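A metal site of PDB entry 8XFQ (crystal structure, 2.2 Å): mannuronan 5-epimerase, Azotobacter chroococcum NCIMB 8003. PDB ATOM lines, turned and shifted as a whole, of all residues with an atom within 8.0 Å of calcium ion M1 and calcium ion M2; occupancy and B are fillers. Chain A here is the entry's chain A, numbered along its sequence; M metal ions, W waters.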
ATOM      1  N   VAL A 330      -3.738  27.916 -11.678  1.00  0.00           N
ATOM      2  CA  VAL A 330      -2.977  26.671 -11.572  1.00  0.00           C
ATOM      3  C   VAL A 330      -1.527  26.968 -11.934  1.00  0.00           C
ATOM      4  O   VAL A 330      -1.217  27.214 -13.103  1.00  0.00           O
ATOM      5  CB  VAL A 330      -3.550  25.565 -12.476  1.00  0.00           C
ATOM      6  CG1 VAL A 330      -2.992  24.216 -12.062  1.00  0.00           C
ATOM      7  CG2 VAL A 330      -5.078  25.540 -12.412  1.00  0.00           C
ATOM      8  N   GLY A 332       1.059  25.240 -12.614  1.00  0.00           N
ATOM      9  CA  GLY A 332       1.595  23.973 -13.063  1.00  0.00           C
ATOM     10  C   GLY A 332       0.711  23.352 -14.111  1.00  0.00           C
ATOM     11  O   GLY A 332      -0.301  23.930 -14.535  1.00  0.00           O
ATOM     12  N   ALA A 333       1.091  22.144 -14.523  1.00  0.00           N
ATOM     13  CA  ALA A 333       0.438  21.479 -15.629  1.00  0.00           C
ATOM     14  C   ALA A 333      -0.902  20.886 -15.204  1.00  0.00           C
ATOM     15  O   ALA A 333      -1.040  20.316 -14.113  1.00  0.00           O
ATOM     16  CB  ALA A 333       1.335  20.376 -16.189  1.00  0.00           C
ATOM     17  N   ALA A 334      -1.892  21.020 -16.074  1.00  0.00           N
ATOM     18  CA  ALA A 334      -3.204  20.413 -15.884  1.00  0.00           C
ATOM     19  C   ALA A 334      -3.425  19.372 -16.967  1.00  0.00           C
ATOM     20  O   ALA A 334      -3.279  19.677 -18.157  1.00  0.00           O
ATOM     21  CB  ALA A 334      -4.311  21.472 -15.922  1.00  0.00           C
ATOM     22  N   ASP A 346     -10.725  24.433 -19.597  1.00  0.00           N
ATOM     23  CA  ASP A 346      -9.803  25.559 -19.676  1.00  0.00           C
ATOM     24  C   ASP A 346      -8.555  25.250 -18.863  1.00  0.00           C
ATOM     25  O   ASP A 346      -8.646  24.915 -17.679  1.00  0.00           O
ATOM     26  CB  ASP A 346     -10.438  26.851 -19.147  1.00  0.00           C
ATOM     27  CG  ASP A 346     -11.747  27.189 -19.834  1.00  0.00           C
ATOM     28  OD1 ASP A 346     -11.949  26.769 -21.000  1.00  0.00           O
ATOM     29  OD2 ASP A 346     -12.560  27.918 -19.221  1.00  0.00           O
ATOM     30  N   GLY A 347      -7.400  25.363 -19.502  1.00  0.00           N
ATOM     31  CA  GLY A 347      -6.137  25.313 -18.810  1.00  0.00           C
ATOM     32  C   GLY A 347      -5.817  26.650 -18.151  1.00  0.00           C
ATOM     33  O   GLY A 347      -6.608  27.587 -18.149  1.00  0.00           O
ATOM     34  N   ALA A 348      -4.618  26.711 -17.594  1.00  0.00           N
ATOM     35  CA  ALA A 348      -4.172  27.878 -16.829  1.00  0.00           C
ATOM     36  C   ALA A 348      -2.698  28.119 -17.181  1.00  0.00           C
ATOM     37  O   ALA A 348      -2.214  27.688 -18.230  1.00  0.00           O
ATOM     38  CB  ALA A 348      -4.427  27.678 -15.330  1.00  0.00           C
ATOM     39  N   ALA A 349      -1.996  28.845 -16.307  1.00  0.00           N
ATOM     40  CA  ALA A 349      -0.629  29.285 -16.582  1.00  0.00           C
ATOM     41  C   ALA A 349       0.324  28.153 -16.984  1.00  0.00           C
ATOM     42  O   ALA A 349       1.373  28.435 -17.578  1.00  0.00           O
ATOM     43  CB  ALA A 349      -0.069  29.997 -15.342  1.00  0.00           C
ATOM     44  N   GLY A 350       0.004  26.892 -16.679  1.00  0.00           N
ATOM     45  CA  GLY A 350       0.932  25.816 -16.949  1.00  0.00           C
ATOM     46  C   GLY A 350       0.885  25.299 -18.384  1.00  0.00           C
ATOM     47  O   GLY A 350       0.069  25.708 -19.203  1.00  0.00           O
ATOM     48  N   ASN A 351       1.801  24.373 -18.674  1.00  0.00           N
ATOM     49  CA  ASN A 351       1.809  23.661 -19.955  1.00  0.00           C
ATOM     50  C   ASN A 351       0.844  22.480 -19.842  1.00  0.00           C
ATOM     51  O   ASN A 351       1.195  21.434 -19.305  1.00  0.00           O
ATOM     52  CB  ASN A 351       3.210  23.184 -20.309  1.00  0.00           C
ATOM     53  CG  ASN A 351       4.160  24.319 -20.643  1.00  0.00           C
ATOM     54  OD1 ASN A 351       3.742  25.471 -20.774  1.00  0.00           O
ATOM     55  ND2 ASN A 351       5.431  23.999 -20.777  1.00  0.00           N
ATOM     56  N   ASP A 352      -0.365  22.653 -20.353  1.00  0.00           N
ATOM     57  CA  ASP A 352      -1.459  21.723 -20.109  1.00  0.00           C
ATOM     58  C   ASP A 352      -1.697  20.804 -21.302  1.00  0.00           C
ATOM     59  O   ASP A 352      -1.336  21.116 -22.439  1.00  0.00           O
ATOM     60  CB  ASP A 352      -2.733  22.491 -19.763  1.00  0.00           C
ATOM     61  CG  ASP A 352      -2.515  23.543 -18.693  1.00  0.00           C
ATOM     62  OD1 ASP A 352      -1.862  23.232 -17.677  1.00  0.00           O
ATOM     63  OD2 ASP A 352      -3.000  24.677 -18.860  1.00  0.00           O
ATOM     64  N   LEU A 353      -2.317  19.660 -21.023  1.00  0.00           N
ATOM     65  CA  LEU A 353      -2.764  18.718 -22.027  1.00  0.00           C
ATOM     66  C   LEU A 353      -4.283  18.667 -22.002  1.00  0.00           C
ATOM     67  O   LEU A 353      -4.879  18.428 -20.940  1.00  0.00           O
ATOM     68  CB  LEU A 353      -2.180  17.326 -21.787  1.00  0.00           C
ATOM     69  CG  LEU A 353      -2.807  16.164 -22.559  1.00  0.00           C
ATOM     70  CD1 LEU A 353      -2.546  16.312 -24.049  1.00  0.00           C
ATOM     71  CD2 LEU A 353      -2.289  14.822 -22.040  1.00  0.00           C
ATOM     72  N   LEU A 354      -4.911  18.878 -23.163  1.00  0.00           N
ATOM     73  CA  LEU A 354      -6.363  18.964 -23.238  1.00  0.00           C
ATOM     74  C   LEU A 354      -6.899  17.984 -24.269  1.00  0.00           C
ATOM     75  O   LEU A 354      -6.392  17.921 -25.398  1.00  0.00           O
ATOM     76  CB  LEU A 354      -6.810  20.393 -23.578  1.00  0.00           C
ATOM     77  CG  LEU A 354      -6.477  21.384 -22.463  1.00  0.00           C
ATOM     78  CD1 LEU A 354      -5.253  22.217 -22.828  1.00  0.00           C
ATOM     79  CD2 LEU A 354      -7.676  22.278 -22.169  1.00  0.00           C
ATOM     80  N   SER A 364      -9.581  25.483 -24.068  1.00  0.00           N
ATOM     81  CA  SER A 364      -8.742  26.672 -24.026  1.00  0.00           C
ATOM     82  C   SER A 364      -7.517  26.373 -23.184  1.00  0.00           C
ATOM     83  O   SER A 364      -7.609  25.685 -22.159  1.00  0.00           O
ATOM     84  CB  SER A 364      -9.509  27.879 -23.451  1.00  0.00           C
ATOM     85  OG  SER A 364      -9.493  27.864 -22.039  1.00  0.00           O
ATOM     86  N   GLY A 365      -6.375  26.886 -23.618  1.00  0.00           N
ATOM     87  CA  GLY A 365      -5.131  26.606 -22.938  1.00  0.00           C
ATOM     88  C   GLY A 365      -4.765  27.604 -21.862  1.00  0.00           C
ATOM     89  O   GLY A 365      -4.178  27.230 -20.843  1.00  0.00           O
ATOM     90  N   GLY A 366      -5.117  28.869 -22.062  1.00  0.00           N
ATOM     91  CA  GLY A 366      -4.613  29.887 -21.158  1.00  0.00           C
ATOM     92  C   GLY A 366      -3.142  30.142 -21.409  1.00  0.00           C
ATOM     93  O   GLY A 366      -2.619  29.931 -22.510  1.00  0.00           O
ATOM     94  N   GLY A 367      -2.445  30.589 -20.365  1.00  0.00           N
ATOM     95  CA  GLY A 367      -1.024  30.866 -20.482  1.00  0.00           C
ATOM     96  C   GLY A 367      -0.212  29.602 -20.716  1.00  0.00           C
ATOM     97  O   GLY A 367      -0.686  28.468 -20.574  1.00  0.00           O
ATOM     98  N   GLY A 368       1.043  29.799 -21.096  1.00  0.00           N
ATOM     99  CA  GLY A 368       1.943  28.685 -21.323  1.00  0.00           C
ATOM    100  C   GLY A 368       1.745  28.016 -22.679  1.00  0.00           C
ATOM    101  O   GLY A 368       0.975  28.471 -23.532  1.00  0.00           O
ATOM    102  N   ALA A 369       2.476  26.921 -22.873  1.00  0.00           N
ATOM    103  CA  ALA A 369       2.441  26.153 -24.120  1.00  0.00           C
ATOM    104  C   ALA A 369       1.603  24.901 -23.890  1.00  0.00           C
ATOM    105  O   ALA A 369       2.022  23.994 -23.148  1.00  0.00           O
ATOM    106  CB  ALA A 369       3.848  25.798 -24.590  1.00  0.00           C
ATOM    107  N   ASP A 370       0.449  24.833 -24.530  1.00  0.00           N
ATOM    108  CA  ASP A 370      -0.528  23.780 -24.276  1.00  0.00           C
ATOM    109  C   ASP A 370      -0.705  22.891 -25.511  1.00  0.00           C
ATOM    110  O   ASP A 370      -0.604  23.348 -26.645  1.00  0.00           O
ATOM    111  CB  ASP A 370      -1.867  24.380 -23.860  1.00  0.00           C
ATOM    112  CG  ASP A 370      -1.733  25.308 -22.681  1.00  0.00           C
ATOM    113  OD1 ASP A 370      -1.306  24.823 -21.601  1.00  0.00           O
ATOM    114  OD2 ASP A 370      -2.017  26.512 -22.825  1.00  0.00           O
ATOM    115  N   THR A 371      -0.983  21.619 -25.246  1.00  0.00           N
ATOM    116  CA  THR A 371      -1.196  20.623 -26.296  1.00  0.00           C
ATOM    117  C   THR A 371      -2.677  20.239 -26.310  1.00  0.00           C
ATOM    118  O   THR A 371      -3.218  19.786 -25.295  1.00  0.00           O
ATOM    119  CB  THR A 371      -0.322  19.388 -26.073  1.00  0.00           C
ATOM    120  OG1 THR A 371       1.056  19.728 -26.265  1.00  0.00           O
ATOM    121  CG2 THR A 371      -0.698  18.279 -27.048  1.00  0.00           C
ATOM    122  N   PHE A 372      -3.324  20.419 -27.461  1.00  0.00           N
ATOM    123  CA  PHE A 372      -4.705  20.006 -27.670  1.00  0.00           C
ATOM    124  C   PHE A 372      -4.691  18.711 -28.462  1.00  0.00           C
ATOM    125  O   PHE A 372      -4.405  18.706 -29.660  1.00  0.00           O
ATOM    126  CB  PHE A 372      -5.496  21.093 -28.387  1.00  0.00           C
ATOM    127  CG  PHE A 372      -5.455  22.432 -27.699  1.00  0.00           C
ATOM    128  CD1 PHE A 372      -4.446  23.336 -27.974  1.00  0.00           C
ATOM    129  CD2 PHE A 372      -6.421  22.770 -26.762  1.00  0.00           C
ATOM    130  CE1 PHE A 372      -4.393  24.562 -27.340  1.00  0.00           C
ATOM    131  CE2 PHE A 372      -6.380  24.002 -26.121  1.00  0.00           C
ATOM    132  CZ  PHE A 372      -5.366  24.899 -26.411  1.00  0.00           C
ATOM    133  N   ASP A 396      -8.331  29.771 -27.745  1.00  0.00           N
ATOM    134  CA  ASP A 396      -7.187  30.680 -27.687  1.00  0.00           C
ATOM    135  C   ASP A 396      -5.929  30.019 -28.229  1.00  0.00           C
ATOM    136  O   ASP A 396      -4.850  30.167 -27.659  1.00  0.00           O
ATOM    137  CB  ASP A 396      -6.952  31.141 -26.250  1.00  0.00           C
ATOM    138  CG  ASP A 396      -6.615  29.994 -25.304  1.00  0.00           C
ATOM    139  OD1 ASP A 396      -6.790  28.815 -25.693  1.00  0.00           O
ATOM    140  OD2 ASP A 396      -6.162  30.267 -24.170  1.00  0.00           O
ATOM    141  N   PHE A 397      -6.033  29.299 -29.348  1.00  0.00           N
ATOM    142  CA  PHE A 397      -4.830  28.655 -29.879  1.00  0.00           C
ATOM    143  C   PHE A 397      -3.804  29.707 -30.272  1.00  0.00           C
ATOM    144  O   PHE A 397      -4.119  30.671 -30.979  1.00  0.00           O
ATOM    145  CB  PHE A 397      -5.158  27.760 -31.076  1.00  0.00           C
ATOM    146  CG  PHE A 397      -3.988  26.940 -31.521  1.00  0.00           C
ATOM    147  CD1 PHE A 397      -3.679  25.747 -30.875  1.00  0.00           C
ATOM    148  CD2 PHE A 397      -3.166  27.358 -32.547  1.00  0.00           C
ATOM    149  CE1 PHE A 397      -2.590  24.985 -31.263  1.00  0.00           C
ATOM    150  CE2 PHE A 397      -2.076  26.598 -32.949  1.00  0.00           C
ATOM    151  CZ  PHE A 397      -1.794  25.413 -32.296  1.00  0.00           C
ATOM    152  N   THR A 398      -2.572  29.515 -29.811  1.00  0.00           N
ATOM    153  CA  THR A 398      -1.514  30.499 -29.966  1.00  0.00           C
ATOM    154  C   THR A 398      -0.444  29.908 -30.872  1.00  0.00           C
ATOM    155  O   THR A 398       0.342  29.048 -30.431  1.00  0.00           O
ATOM    156  CB  THR A 398      -0.929  30.883 -28.603  1.00  0.00           C
ATOM    157  OG1 THR A 398      -1.841  31.761 -27.932  1.00  0.00           O
ATOM    158  CG2 THR A 398       0.389  31.624 -28.771  1.00  0.00           C
ATOM    159  N   ALA A 401       3.394  28.670 -29.990  1.00  0.00           N
ATOM    160  CA  ALA A 401       3.474  28.213 -28.606  1.00  0.00           C
ATOM    161  C   ALA A 401       2.694  26.931 -28.361  1.00  0.00           C
ATOM    162  O   ALA A 401       3.250  25.970 -27.835  1.00  0.00           O
ATOM    163  CB  ALA A 401       2.979  29.319 -27.658  1.00  0.00           C
ATOM    164  N   ASP A 402       1.414  26.897 -28.736  1.00  0.00           N
ATOM    165  CA  ASP A 402       0.585  25.726 -28.497  1.00  0.00           C
ATOM    166  C   ASP A 402       0.823  24.676 -29.588  1.00  0.00           C
ATOM    167  O   ASP A 402       1.561  24.885 -30.557  1.00  0.00           O
ATOM    168  CB  ASP A 402      -0.881  26.115 -28.427  1.00  0.00           C
ATOM    169  CG  ASP A 402      -1.176  27.092 -27.298  1.00  0.00           C
ATOM    170  OD1 ASP A 402      -0.434  27.087 -26.292  1.00  0.00           O
ATOM    171  OD2 ASP A 402      -2.153  27.852 -27.415  1.00  0.00           O
ATOM    172  N   LEU A 403       0.188  23.510 -29.419  1.00  0.00           N
ATOM    173  CA  LEU A 403       0.326  22.415 -30.359  1.00  0.00           C
ATOM    174  C   LEU A 403      -0.993  21.673 -30.498  1.00  0.00           C
ATOM    175  O   LEU A 403      -1.669  21.402 -29.495  1.00  0.00           O
ATOM    176  CB  LEU A 403       1.432  21.439 -29.934  1.00  0.00           C
ATOM    177  CG  LEU A 403       1.651  20.224 -30.837  1.00  0.00           C
ATOM    178  CD1 LEU A 403       2.271  20.635 -32.157  1.00  0.00           C
ATOM    179  CD2 LEU A 403       2.507  19.168 -30.127  1.00  0.00           C
ATOM    180  N   THR A 476       4.525  19.899 -26.018  1.00  0.00           N
ATOM    181  CA  THR A 476       4.706  20.974 -25.056  1.00  0.00           C
ATOM    182  C   THR A 476       4.620  20.502 -23.608  1.00  0.00           C
ATOM    183  O   THR A 476       4.828  21.306 -22.693  1.00  0.00           O
ATOM    184  CB  THR A 476       3.666  22.077 -25.284  1.00  0.00           C
ATOM    185  OG1 THR A 476       2.419  21.673 -24.725  1.00  0.00           O
ATOM    186  CG2 THR A 476       3.504  22.349 -26.773  1.00  0.00           C
HETATM  187 CA    CA M   1      -1.326  28.564 -24.265  1.00  0.00          CA
HETATM  188 CA    CA M   2      -2.019  26.525 -20.192  1.00  0.00          CA
HETATM  189  O   HOH W   1      -3.807  28.213 -25.509  1.00  0.00           O
HETATM  190  O   HOH W   2      -0.938  31.016 -25.359  1.00  0.00           O
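The side-chain carboxylate (OD1) of Asp 352 is in hydrogen-bond range of the backbone NH (N) of Ala 334 (2.7 Å).
The backbone NH (N) of Gly 365 lies within hydrogen-bond range of the side-chain carboxylate (OD1) of Asp 396 (2.9 Å).
The backbone carbonyl oxygen of Asp 370 is in hydrogen-bond range of the backbone NH of Leu 403 (2.9 Å).
The side-chain carboxylate of Asp 402 is in hydrogen-bond range of the backbone NH of Thr 398 (2.9 Å).
O of Asp 352 is in hydrogen-bond range of N of Thr 371.
N of Gly 366 sits at hydrogen-bond distance from OD2 of Asp 396, 2.7 Å away.
The nearest printed residue that does not touch calcium ion M1 is Gly 365 (4.3 Å).
Seven residues have an atom within 4 Å of calcium ion M2: Ala 348, Gly 350, Asp 352, Gly 365, Gly 366, Gly 367 and Asp 370.
The nearest printed residue that does not touch calcium ion M2 is Ala 349 (4.3 Å).
The backbone carbonyl oxygen (O) of Gly 368 is bound to calcium ion M1 (2.4 Å).
O of Gly 366 binds calcium ion M1.
OD2 of Asp 370 binds calcium ion M1, at 2.6 Å.
OD1 of Asp 402 is bound to calcium ion M1 (2.7 Å).
Water W2 binds calcium ion M1, at 2.7 Å.
Water W1 is bound to calcium ion M1 (2.8 Å).
Calcium ion M1 has six donor atoms within binding distance.
Calcium ion M2 is bound by O of Ala 348 (2.3 Å), OD1 of Asp 370 (2.3 Å), O of Gly 365 (2.4 Å), O of Gly 367 (2.4 Å), O of Gly 350 (2.5 Å), OD2 of Asp 352 (2.5 Å) and OD2 of Asp 370 (2.6 Å).
Water W1 lies within hydrogen-bond range of OD2 of Asp 402 (2.5 Å), OD1 of Asp 396 (3.0 Å) and N of Gly 365 (3.5 Å).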
